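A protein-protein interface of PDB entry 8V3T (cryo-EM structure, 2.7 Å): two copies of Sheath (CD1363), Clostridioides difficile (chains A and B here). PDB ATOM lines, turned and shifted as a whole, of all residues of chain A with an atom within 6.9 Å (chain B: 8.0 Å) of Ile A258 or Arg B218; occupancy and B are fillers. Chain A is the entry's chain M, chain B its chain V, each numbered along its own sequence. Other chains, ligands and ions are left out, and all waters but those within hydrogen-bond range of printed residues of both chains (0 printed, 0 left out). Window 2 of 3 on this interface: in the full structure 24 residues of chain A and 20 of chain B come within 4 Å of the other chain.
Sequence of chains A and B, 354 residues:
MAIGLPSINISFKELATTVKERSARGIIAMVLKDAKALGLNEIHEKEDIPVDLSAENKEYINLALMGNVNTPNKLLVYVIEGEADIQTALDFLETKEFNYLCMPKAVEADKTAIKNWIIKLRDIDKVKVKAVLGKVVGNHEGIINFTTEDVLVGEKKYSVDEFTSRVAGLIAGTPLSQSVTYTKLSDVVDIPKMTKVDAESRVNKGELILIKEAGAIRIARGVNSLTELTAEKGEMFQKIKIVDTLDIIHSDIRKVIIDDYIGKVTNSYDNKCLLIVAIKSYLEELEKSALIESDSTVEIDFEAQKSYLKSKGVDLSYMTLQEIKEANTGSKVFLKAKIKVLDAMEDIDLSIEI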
ATOM      1  N   ILE A 253      36.694  -0.518  27.353  1.00  0.00           N
ATOM      2  CA  ILE A 253      37.213   0.096  28.572  1.00  0.00           C
ATOM      3  C   ILE A 253      36.740   1.541  28.680  1.00  0.00           C
ATOM      4  O   ILE A 253      36.360   2.011  29.764  1.00  0.00           O
ATOM      5  CB  ILE A 253      38.748  -0.015  28.620  1.00  0.00           C
ATOM      6  CG1 ILE A 253      39.159  -1.459  28.904  1.00  0.00           C
ATOM      7  CG2 ILE A 253      39.313   0.892  29.697  1.00  0.00           C
ATOM      8  CD1 ILE A 253      40.631  -1.635  29.196  1.00  0.00           C
ATOM      9  N   ARG A 254      36.748   2.268  27.558  1.00  0.00           N
ATOM     10  CA  ARG A 254      36.209   3.624  27.563  1.00  0.00           C
ATOM     11  C   ARG A 254      34.745   3.630  27.977  1.00  0.00           C
ATOM     12  O   ARG A 254      34.311   4.505  28.734  1.00  0.00           O
ATOM     13  CB  ARG A 254      36.375   4.265  26.188  1.00  0.00           C
ATOM     14  CG  ARG A 254      36.597   5.763  26.235  1.00  0.00           C
ATOM     15  CD  ARG A 254      36.936   6.312  24.863  1.00  0.00           C
ATOM     16  NE  ARG A 254      36.315   7.612  24.638  1.00  0.00           N
ATOM     17  CZ  ARG A 254      35.437   7.865  23.679  1.00  0.00           C
ATOM     18  NH1 ARG A 254      35.052   6.927  22.829  1.00  0.00           N
ATOM     19  NH2 ARG A 254      34.929   9.089  23.570  1.00  0.00           N
ATOM     20  N   LYS A 255      33.967   2.660  27.489  1.00  0.00           N
ATOM     21  CA  LYS A 255      32.556   2.597  27.853  1.00  0.00           C
ATOM     22  C   LYS A 255      32.375   2.457  29.358  1.00  0.00           C
ATOM     23  O   LYS A 255      31.599   3.202  29.967  1.00  0.00           O
ATOM     24  CB  LYS A 255      31.865   1.445  27.125  1.00  0.00           C
ATOM     25  CG  LYS A 255      31.060   1.872  25.914  1.00  0.00           C
ATOM     26  CD  LYS A 255      30.059   0.797  25.528  1.00  0.00           C
ATOM     27  CE  LYS A 255      29.186   1.241  24.370  1.00  0.00           C
ATOM     28  NZ  LYS A 255      28.214   0.183  23.981  1.00  0.00           N
ATOM     29  N   VAL A 256      33.082   1.507  29.980  1.00  0.00           N
ATOM     30  CA  VAL A 256      32.884   1.321  31.421  1.00  0.00           C
ATOM     31  C   VAL A 256      33.329   2.564  32.185  1.00  0.00           C
ATOM     32  O   VAL A 256      32.620   3.050  33.084  1.00  0.00           O
ATOM     33  CB  VAL A 256      33.594   0.053  31.940  1.00  0.00           C
ATOM     34  CG1 VAL A 256      34.742  -0.341  31.059  1.00  0.00           C
ATOM     35  CG2 VAL A 256      34.063   0.242  33.379  1.00  0.00           C
ATOM     36  N   ILE A 257      34.494   3.118  31.825  1.00  0.00           N
ATOM     37  CA  ILE A 257      35.023   4.272  32.551  1.00  0.00           C
ATOM     38  C   ILE A 257      34.059   5.448  32.464  1.00  0.00           C
ATOM     39  O   ILE A 257      33.769   6.112  33.466  1.00  0.00           O
ATOM     40  CB  ILE A 257      36.419   4.649  32.024  1.00  0.00           C
ATOM     41  CG1 ILE A 257      37.447   3.589  32.423  1.00  0.00           C
ATOM     42  CG2 ILE A 257      36.834   6.013  32.542  1.00  0.00           C
ATOM     43  CD1 ILE A 257      38.867   3.949  32.050  1.00  0.00           C
ATOM     44  N   ILE A 258      33.546   5.724  31.263  1.00  0.00           N
ATOM     45  CA  ILE A 258      32.622   6.841  31.094  1.00  0.00           C
ATOM     46  C   ILE A 258      31.317   6.577  31.835  1.00  0.00           C
ATOM     47  O   ILE A 258      30.756   7.479  32.469  1.00  0.00           O
ATOM     48  CB  ILE A 258      32.385   7.110  29.598  1.00  0.00           C
ATOM     49  CG1 ILE A 258      33.599   7.815  28.992  1.00  0.00           C
ATOM     50  CG2 ILE A 258      31.129   7.938  29.389  1.00  0.00           C
ATOM     51  CD1 ILE A 258      33.418   8.201  27.546  1.00  0.00           C
ATOM     52  N   ASP A 259      30.816   5.340  31.778  1.00  0.00           N
ATOM     53  CA  ASP A 259      29.520   5.043  32.374  1.00  0.00           C
ATOM     54  C   ASP A 259      29.541   5.200  33.889  1.00  0.00           C
ATOM     55  O   ASP A 259      28.584   5.718  34.475  1.00  0.00           O
ATOM     56  CB  ASP A 259      29.080   3.629  31.997  1.00  0.00           C
ATOM     57  CG  ASP A 259      28.403   3.571  30.645  1.00  0.00           C
ATOM     58  OD1 ASP A 259      28.127   4.646  30.069  1.00  0.00           O
ATOM     59  OD2 ASP A 259      28.145   2.451  30.157  1.00  0.00           O
ATOM     60  N   ASP A 260      30.616   4.759  34.549  1.00  0.00           N
ATOM     61  CA  ASP A 260      30.543   4.591  35.995  1.00  0.00           C
ATOM     62  C   ASP A 260      31.395   5.548  36.821  1.00  0.00           C
ATOM     63  O   ASP A 260      31.177   5.630  38.034  1.00  0.00           O
ATOM     64  CB  ASP A 260      30.912   3.149  36.374  1.00  0.00           C
ATOM     65  CG  ASP A 260      30.104   2.123  35.611  1.00  0.00           C
ATOM     66  OD1 ASP A 260      28.863   2.252  35.576  1.00  0.00           O
ATOM     67  OD2 ASP A 260      30.708   1.188  35.045  1.00  0.00           O
ATOM     68  N   TYR A 261      32.346   6.274  36.231  1.00  0.00           N
ATOM     69  CA  TYR A 261      33.317   6.988  37.055  1.00  0.00           C
ATOM     70  C   TYR A 261      33.548   8.451  36.703  1.00  0.00           C
ATOM     71  O   TYR A 261      33.987   9.201  37.584  1.00  0.00           O
ATOM     72  CB  TYR A 261      34.669   6.260  37.031  1.00  0.00           C
ATOM     73  CG  TYR A 261      34.620   4.917  37.716  1.00  0.00           C
ATOM     74  CD1 TYR A 261      34.266   3.772  37.017  1.00  0.00           C
ATOM     75  CD2 TYR A 261      34.908   4.795  39.066  1.00  0.00           C
ATOM     76  CE1 TYR A 261      34.209   2.544  37.640  1.00  0.00           C
ATOM     77  CE2 TYR A 261      34.854   3.571  39.699  1.00  0.00           C
ATOM     78  CZ  TYR A 261      34.504   2.449  38.981  1.00  0.00           C
ATOM     79  OH  TYR A 261      34.450   1.228  39.606  1.00  0.00           O
ATOM     80  N   ILE A 262      33.277   8.895  35.480  1.00  0.00           N
ATOM     81  CA  ILE A 262      33.576  10.274  35.102  1.00  0.00           C
ATOM     82  C   ILE A 262      32.527  11.187  35.728  1.00  0.00           C
ATOM     83  O   ILE A 262      31.354  11.158  35.348  1.00  0.00           O
ATOM     84  CB  ILE A 262      33.627  10.447  33.581  1.00  0.00           C
ATOM     85  CG1 ILE A 262      34.725   9.568  32.983  1.00  0.00           C
ATOM     86  CG2 ILE A 262      33.860  11.906  33.225  1.00  0.00           C
ATOM     87  CD1 ILE A 262      36.123  10.051  33.287  1.00  0.00           C
ATOM     88  N   GLY A 263      32.949  11.999  36.695  1.00  0.00           N
ATOM     89  CA  GLY A 263      32.069  12.945  37.345  1.00  0.00           C
ATOM     90  C   GLY A 263      31.153  12.364  38.398  1.00  0.00           C
ATOM     91  O   GLY A 263      30.333  13.103  38.957  1.00  0.00           O
ATOM     92  N   LYS A 264      31.261  11.069  38.693  1.00  0.00           N
ATOM     93  CA  LYS A 264      30.356  10.428  39.639  1.00  0.00           C
ATOM     94  C   LYS A 264      30.933  10.342  41.047  1.00  0.00           C
ATOM     95  O   LYS A 264      30.185  10.450  42.024  1.00  0.00           O
ATOM     96  CB  LYS A 264      29.993   9.024  39.150  1.00  0.00           C
ATOM     97  CG  LYS A 264      29.504   8.964  37.715  1.00  0.00           C
ATOM     98  CD  LYS A 264      28.224   9.757  37.531  1.00  0.00           C
ATOM     99  CE  LYS A 264      27.739   9.685  36.094  1.00  0.00           C
ATOM    100  NZ  LYS A 264      28.781  10.146  35.135  1.00  0.00           N
ATOM    101  N   THR B 148      25.293  27.538  23.505  1.00  0.00           N
ATOM    102  CA  THR B 148      25.049  26.507  22.504  1.00  0.00           C
ATOM    103  C   THR B 148      23.852  26.926  21.667  1.00  0.00           C
ATOM    104  O   THR B 148      22.793  27.253  22.212  1.00  0.00           O
ATOM    105  CB  THR B 148      24.807  25.137  23.152  1.00  0.00           C
ATOM    106  OG1 THR B 148      26.065  24.504  23.411  1.00  0.00           O
ATOM    107  CG2 THR B 148      23.989  24.245  22.233  1.00  0.00           C
ATOM    108  N   LEU B 170      19.014  21.002  35.103  1.00  0.00           N
ATOM    109  CA  LEU B 170      20.048  19.973  35.144  1.00  0.00           C
ATOM    110  C   LEU B 170      21.004  20.208  36.306  1.00  0.00           C
ATOM    111  O   LEU B 170      21.334  19.282  37.054  1.00  0.00           O
ATOM    112  CB  LEU B 170      20.821  19.958  33.825  1.00  0.00           C
ATOM    113  CG  LEU B 170      20.422  18.967  32.732  1.00  0.00           C
ATOM    114  CD1 LEU B 170      21.533  18.865  31.704  1.00  0.00           C
ATOM    115  CD2 LEU B 170      20.106  17.607  33.318  1.00  0.00           C
ATOM    116  N   VAL B 180      28.502  17.860  36.991  1.00  0.00           N
ATOM    117  CA  VAL B 180      27.760  17.875  35.734  1.00  0.00           C
ATOM    118  C   VAL B 180      28.639  17.569  34.529  1.00  0.00           C
ATOM    119  O   VAL B 180      28.143  17.589  33.395  1.00  0.00           O
ATOM    120  CB  VAL B 180      27.055  19.230  35.523  1.00  0.00           C
ATOM    121  CG1 VAL B 180      26.106  19.518  36.674  1.00  0.00           C
ATOM    122  CG2 VAL B 180      28.075  20.346  35.371  1.00  0.00           C
ATOM    123  N   THR B 181      29.924  17.291  34.734  1.00  0.00           N
ATOM    124  CA  THR B 181      30.807  16.970  33.622  1.00  0.00           C
ATOM    125  C   THR B 181      30.383  15.662  32.964  1.00  0.00           C
ATOM    126  O   THR B 181      30.157  14.655  33.643  1.00  0.00           O
ATOM    127  CB  THR B 181      32.254  16.876  34.107  1.00  0.00           C
ATOM    128  OG1 THR B 181      32.659  18.141  34.644  1.00  0.00           O
ATOM    129  CG2 THR B 181      33.179  16.505  32.960  1.00  0.00           C
ATOM    130  N   TYR B 182      30.265  15.688  31.635  1.00  0.00           N
ATOM    131  CA  TYR B 182      29.883  14.537  30.820  1.00  0.00           C
ATOM    132  C   TYR B 182      28.492  14.011  31.157  1.00  0.00           C
ATOM    133  O   TYR B 182      28.193  12.837  30.911  1.00  0.00           O
ATOM    134  CB  TYR B 182      30.913  13.407  30.925  1.00  0.00           C
ATOM    135  CG  TYR B 182      31.948  13.424  29.824  1.00  0.00           C
ATOM    136  CD1 TYR B 182      32.573  14.606  29.450  1.00  0.00           C
ATOM    137  CD2 TYR B 182      32.300  12.260  29.157  1.00  0.00           C
ATOM    138  CE1 TYR B 182      33.518  14.626  28.445  1.00  0.00           C
ATOM    139  CE2 TYR B 182      33.244  12.270  28.151  1.00  0.00           C
ATOM    140  CZ  TYR B 182      33.850  13.456  27.799  1.00  0.00           C
ATOM    141  OH  TYR B 182      34.794  13.472  26.797  1.00  0.00           O
ATOM    142  N   THR B 183      27.627  14.852  31.718  1.00  0.00           N
ATOM    143  CA  THR B 183      26.243  14.465  31.954  1.00  0.00           C
ATOM    144  C   THR B 183      25.476  14.497  30.639  1.00  0.00           C
ATOM    145  O   THR B 183      25.527  15.489  29.905  1.00  0.00           O
ATOM    146  CB  THR B 183      25.591  15.397  32.973  1.00  0.00           C
ATOM    147  OG1 THR B 183      26.342  15.369  34.194  1.00  0.00           O
ATOM    148  CG2 THR B 183      24.163  14.964  33.254  1.00  0.00           C
ATOM    149  N   LYS B 184      24.756  13.419  30.346  1.00  0.00           N
ATOM    150  CA  LYS B 184      24.109  13.239  29.056  1.00  0.00           C
ATOM    151  C   LYS B 184      22.636  13.617  29.126  1.00  0.00           C
ATOM    152  O   LYS B 184      21.978  13.419  30.151  1.00  0.00           O
ATOM    153  CB  LYS B 184      24.254  11.794  28.575  1.00  0.00           C
ATOM    154  CG  LYS B 184      23.636  10.761  29.502  1.00  0.00           C
ATOM    155  CD  LYS B 184      23.805   9.356  28.952  1.00  0.00           C
ATOM    156  CE  LYS B 184      23.144   9.209  27.596  1.00  0.00           C
ATOM    157  NZ  LYS B 184      23.155   7.795  27.130  1.00  0.00           N
ATOM    158  N   LEU B 185      22.126  14.170  28.026  1.00  0.00           N
ATOM    159  CA  LEU B 185      20.722  14.548  27.893  1.00  0.00           C
ATOM    160  C   LEU B 185      20.083  13.646  26.844  1.00  0.00           C
ATOM    161  O   LEU B 185      20.406  13.742  25.655  1.00  0.00           O
ATOM    162  CB  LEU B 185      20.575  16.019  27.511  1.00  0.00           C
ATOM    163  CG  LEU B 185      21.256  17.095  28.362  1.00  0.00           C
ATOM    164  CD1 LEU B 185      22.702  17.317  27.945  1.00  0.00           C
ATOM    165  CD2 LEU B 185      20.471  18.393  28.279  1.00  0.00           C
ATOM    166  N   SER B 186      19.171  12.777  27.285  1.00  0.00           N
ATOM    167  CA  SER B 186      18.523  11.853  26.361  1.00  0.00           C
ATOM    168  C   SER B 186      17.485  12.550  25.491  1.00  0.00           C
ATOM    169  O   SER B 186      17.301  12.173  24.329  1.00  0.00           O
ATOM    170  CB  SER B 186      17.876  10.705  27.137  1.00  0.00           C
ATOM    171  OG  SER B 186      17.147   9.852  26.271  1.00  0.00           O
ATOM    172  N   VAL B 188      17.487  15.595  24.228  1.00  0.00           N
ATOM    173  CA  VAL B 188      18.081  16.365  23.143  1.00  0.00           C
ATOM    174  C   VAL B 188      18.471  15.431  22.006  1.00  0.00           C
ATOM    175  O   VAL B 188      18.952  14.311  22.233  1.00  0.00           O
ATOM    176  CB  VAL B 188      19.292  17.161  23.657  1.00  0.00           C
ATOM    177  CG1 VAL B 188      19.851  18.034  22.561  1.00  0.00           C
ATOM    178  CG2 VAL B 188      18.902  18.003  24.859  1.00  0.00           C
ATOM    179  N   ILE B 191      22.628  18.646  17.600  1.00  0.00           N
ATOM    180  CA  ILE B 191      23.365  19.885  17.851  1.00  0.00           C
ATOM    181  C   ILE B 191      24.092  20.265  16.566  1.00  0.00           C
ATOM    182  O   ILE B 191      24.564  19.376  15.843  1.00  0.00           O
ATOM    183  CB  ILE B 191      24.344  19.732  19.033  1.00  0.00           C
ATOM    184  CG1 ILE B 191      23.654  20.000  20.373  1.00  0.00           C
ATOM    185  CG2 ILE B 191      25.559  20.638  18.889  1.00  0.00           C
ATOM    186  CD1 ILE B 191      22.720  18.926  20.817  1.00  0.00           C
ATOM    187  N   ILE B 209      29.365  24.678  27.534  1.00  0.00           N
ATOM    188  CA  ILE B 209      28.802  24.370  26.228  1.00  0.00           C
ATOM    189  C   ILE B 209      28.458  22.889  26.148  1.00  0.00           C
ATOM    190  O   ILE B 209      28.920  22.068  26.944  1.00  0.00           O
ATOM    191  CB  ILE B 209      29.749  24.807  25.079  1.00  0.00           C
ATOM    192  CG1 ILE B 209      31.126  24.115  25.114  1.00  0.00           C
ATOM    193  CG2 ILE B 209      29.943  26.312  25.101  1.00  0.00           C
ATOM    194  CD1 ILE B 209      31.187  22.655  24.690  1.00  0.00           C
ATOM    195  N   LEU B 210      27.624  22.558  25.169  1.00  0.00           N
ATOM    196  CA  LEU B 210      27.294  21.176  24.862  1.00  0.00           C
ATOM    197  C   LEU B 210      28.285  20.621  23.848  1.00  0.00           C
ATOM    198  O   LEU B 210      28.724  21.322  22.933  1.00  0.00           O
ATOM    199  CB  LEU B 210      25.871  21.067  24.314  1.00  0.00           C
ATOM    200  CG  LEU B 210      24.735  21.073  25.335  1.00  0.00           C
ATOM    201  CD1 LEU B 210      23.392  20.959  24.636  1.00  0.00           C
ATOM    202  CD2 LEU B 210      24.916  19.947  26.337  1.00  0.00           C
ATOM    203  N   ILE B 211      28.634  19.349  24.020  1.00  0.00           N
ATOM    204  CA  ILE B 211      29.581  18.680  23.141  1.00  0.00           C
ATOM    205  C   ILE B 211      28.977  17.346  22.724  1.00  0.00           C
ATOM    206  O   ILE B 211      28.178  16.749  23.453  1.00  0.00           O
ATOM    207  CB  ILE B 211      30.961  18.493  23.821  1.00  0.00           C
ATOM    208  CG1 ILE B 211      32.089  18.974  22.903  1.00  0.00           C
ATOM    209  CG2 ILE B 211      31.187  17.045  24.234  1.00  0.00           C
ATOM    210  CD1 ILE B 211      32.244  18.185  21.627  1.00  0.00           C
ATOM    211  N   LYS B 212      29.340  16.894  21.528  1.00  0.00           N
ATOM    212  CA  LYS B 212      28.797  15.668  20.959  1.00  0.00           C
ATOM    213  C   LYS B 212      29.855  14.574  21.041  1.00  0.00           C
ATOM    214  O   LYS B 212      30.917  14.684  20.422  1.00  0.00           O
ATOM    215  CB  LYS B 212      28.350  15.898  19.517  1.00  0.00           C
ATOM    216  CG  LYS B 212      27.319  14.906  19.027  1.00  0.00           C
ATOM    217  CD  LYS B 212      26.491  15.510  17.905  1.00  0.00           C
ATOM    218  CE  LYS B 212      25.526  14.500  17.319  1.00  0.00           C
ATOM    219  NZ  LYS B 212      25.241  13.384  18.262  1.00  0.00           N
ATOM    220  N   GLU B 213      29.559  13.527  21.802  1.00  0.00           N
ATOM    221  CA  GLU B 213      30.489  12.436  22.057  1.00  0.00           C
ATOM    222  C   GLU B 213      29.871  11.121  21.583  1.00  0.00           C
ATOM    223  O   GLU B 213      28.822  11.102  20.933  1.00  0.00           O
ATOM    224  CB  GLU B 213      30.859  12.386  23.541  1.00  0.00           C
ATOM    225  CG  GLU B 213      32.311  12.034  23.806  1.00  0.00           C
ATOM    226  CD  GLU B 213      33.274  12.956  23.088  1.00  0.00           C
ATOM    227  OE1 GLU B 213      33.082  14.189  23.151  1.00  0.00           O
ATOM    228  OE2 GLU B 213      34.223  12.447  22.457  1.00  0.00           O
ATOM    229  N   ALA B 214      30.542  10.016  21.905  1.00  0.00           N
ATOM    230  CA  ALA B 214      30.046   8.696  21.540  1.00  0.00           C
ATOM    231  C   ALA B 214      28.709   8.433  22.217  1.00  0.00           C
ATOM    232  O   ALA B 214      28.647   8.258  23.439  1.00  0.00           O
ATOM    233  CB  ALA B 214      31.060   7.615  21.916  1.00  0.00           C
ATOM    234  N   GLY B 215      27.637   8.399  21.432  1.00  0.00           N
ATOM    235  CA  GLY B 215      26.304   8.265  21.984  1.00  0.00           C
ATOM    236  C   GLY B 215      25.556   9.581  22.030  1.00  0.00           C
ATOM    237  O   GLY B 215      25.691  10.412  21.129  1.00  0.00           O
ATOM    238  N   ALA B 216      24.765   9.782  23.081  1.00  0.00           N
ATOM    239  CA  ALA B 216      23.939  10.975  23.193  1.00  0.00           C
ATOM    240  C   ALA B 216      24.798  12.212  23.453  1.00  0.00           C
ATOM    241  O   ALA B 216      26.014  12.140  23.653  1.00  0.00           O
ATOM    242  CB  ALA B 216      22.905  10.804  24.304  1.00  0.00           C
ATOM    243  N   ILE B 217      24.136  13.372  23.437  1.00  0.00           N
ATOM    244  CA  ILE B 217      24.807  14.633  23.724  1.00  0.00           C
ATOM    245  C   ILE B 217      25.129  14.707  25.212  1.00  0.00           C
ATOM    246  O   ILE B 217      24.415  14.152  26.054  1.00  0.00           O
ATOM    247  CB  ILE B 217      23.922  15.817  23.292  1.00  0.00           C
ATOM    248  CG1 ILE B 217      23.295  15.544  21.927  1.00  0.00           C
ATOM    249  CG2 ILE B 217      24.736  17.100  23.242  1.00  0.00           C
ATOM    250  CD1 ILE B 217      24.289  15.439  20.807  1.00  0.00           C
ATOM    251  N   ARG B 218      26.216  15.402  25.546  1.00  0.00           N
ATOM    252  CA  ARG B 218      26.600  15.551  26.941  1.00  0.00           C
ATOM    253  C   ARG B 218      27.366  16.852  27.131  1.00  0.00           C
ATOM    254  O   ARG B 218      27.931  17.410  26.186  1.00  0.00           O
ATOM    255  CB  ARG B 218      27.435  14.360  27.424  1.00  0.00           C
ATOM    256  CG  ARG B 218      28.253  13.688  26.338  1.00  0.00           C
ATOM    257  CD  ARG B 218      29.364  12.847  26.936  1.00  0.00           C
ATOM    258  NE  ARG B 218      28.843  11.848  27.861  1.00  0.00           N
ATOM    259  CZ  ARG B 218      28.550  10.600  27.526  1.00  0.00           C
ATOM    260  NH1 ARG B 218      28.720  10.158  26.291  1.00  0.00           N
ATOM    261  NH2 ARG B 218      28.072   9.774  28.453  1.00  0.00           N
ATOM    262  N   ILE B 219      27.380  17.326  28.378  1.00  0.00           N
ATOM    263  CA  ILE B 219      28.086  18.555  28.716  1.00  0.00           C
ATOM    264  C   ILE B 219      29.587  18.305  28.694  1.00  0.00           C
ATOM    265  O   ILE B 219      30.068  17.254  29.136  1.00  0.00           O
ATOM    266  CB  ILE B 219      27.624  19.073  30.088  1.00  0.00           C
ATOM    267  CG1 ILE B 219      26.101  19.206  30.120  1.00  0.00           C
ATOM    268  CG2 ILE B 219      28.276  20.408  30.412  1.00  0.00           C
ATOM    269  CD1 ILE B 219      25.477  18.755  31.418  1.00  0.00           C
ATOM    270  N   ALA B 220      30.339  19.277  28.177  1.00  0.00           N
ATOM    271  CA  ALA B 220      31.784  19.109  28.058  1.00  0.00           C
ATOM    272  C   ALA B 220      32.466  19.220  29.416  1.00  0.00           C
ATOM    273  O   ALA B 220      33.103  18.271  29.885  1.00  0.00           O
ATOM    274  CB  ALA B 220      32.353  20.140  27.082  1.00  0.00           C
ATOM    275  N   ARG B 221      32.339  20.374  30.065  1.00  0.00           N
ATOM    276  CA  ARG B 221      33.018  20.619  31.327  1.00  0.00           C
ATOM    277  C   ARG B 221      32.121  21.487  32.198  1.00  0.00           C
ATOM    278  O   ARG B 221      31.280  22.235  31.693  1.00  0.00           O
ATOM    279  CB  ARG B 221      34.381  21.287  31.098  1.00  0.00           C
ATOM    280  CG  ARG B 221      35.246  21.428  32.340  1.00  0.00           C
ATOM    281  CD  ARG B 221      35.860  20.099  32.736  1.00  0.00           C
ATOM    282  NE  ARG B 221      37.315  20.129  32.662  1.00  0.00           N
ATOM    283  CZ  ARG B 221      38.092  19.057  32.741  1.00  0.00           C
ATOM    284  NH1 ARG B 221      37.584  17.846  32.896  1.00  0.00           N
ATOM    285  NH2 ARG B 221      39.411  19.205  32.665  1.00  0.00           N
ATOM    286  N   ILE B 348      41.745  10.558  33.057  1.00  0.00           N
ATOM    287  CA  ILE B 348      42.337   9.248  33.301  1.00  0.00           C
ATOM    288  C   ILE B 348      43.371   8.962  32.222  1.00  0.00           C
ATOM    289  O   ILE B 348      43.100   9.147  31.032  1.00  0.00           O
ATOM    290  CB  ILE B 348      41.267   8.138  33.331  1.00  0.00           C
ATOM    291  CG1 ILE B 348      40.357   8.312  34.546  1.00  0.00           C
ATOM    292  CG2 ILE B 348      41.918   6.764  33.338  1.00  0.00           C
ATOM    293  CD1 ILE B 348      39.475   7.125  34.824  1.00  0.00           C
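The side-chain carboxylate of Glu B213 is in salt-bridge range of the guanidinium group of Arg A254 (3.6 Å).
NH1 of Arg B218 is in hydrogen-bond range of O of Ala B214. The backbone carbonyl oxygen (O) of Tyr B182 lies within hydrogen-bond range of the guanidinium group (NE) of Arg B218 (3.3 Å). N of Ile B211 is in hydrogen-bond range of O of Arg B218 (3.0 Å). The backbone carbonyl oxygen of Ile A257 is in hydrogen-bond range of the backbone NH of Ile A262 (3.5 Å).
Ile A257 touches Ile B348 (CG2 to CD1, 3.7 Å). Ile A258 touches Arg B218 (CG2 to NH2, 3.7 Å).
Ile A258 touches one residue of chain B. Arg B218 touches just one residue of chain A: Ile A258 (3.7 Å). Of the printed residues of chain A, Ile B348 touches Ile A257 (3.7 Å). Printed residues of chain B within 4 Å of Ile A257: Ile B348. Of the printed residues of chain A, Glu B213 touches Arg A254 (3.6 Å). Of the printed residues of chain B, Arg A254 touches Glu B213.
Of the 12 printed residues of chain A, 3 touch a printed residue of chain B. Hydrophobic or aromatic side chains of chain A that line the printed part of chain B: Ile A257 and Ile A258. Along chain A the printed residues that touch a printed residue of chain B span positions 254 to 258. Printed residues of chain B that touch a printed residue of chain A: Glu B213, Arg B218 and Ile B348. Hydrophobic or aromatic side chains of chain B that line the printed part of chain A: Ile B348. Among the printed residues, Asp or Glu carboxylates within 4 Å of a Lys or Arg side-chain nitrogen of the other chain: Arg A254 with Glu B213 (3.6 Å).
No position is printed for both chains. Of the 3 pairs that touch across the chains among the printed residues, none has its exchanged pair printed and touching as well.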
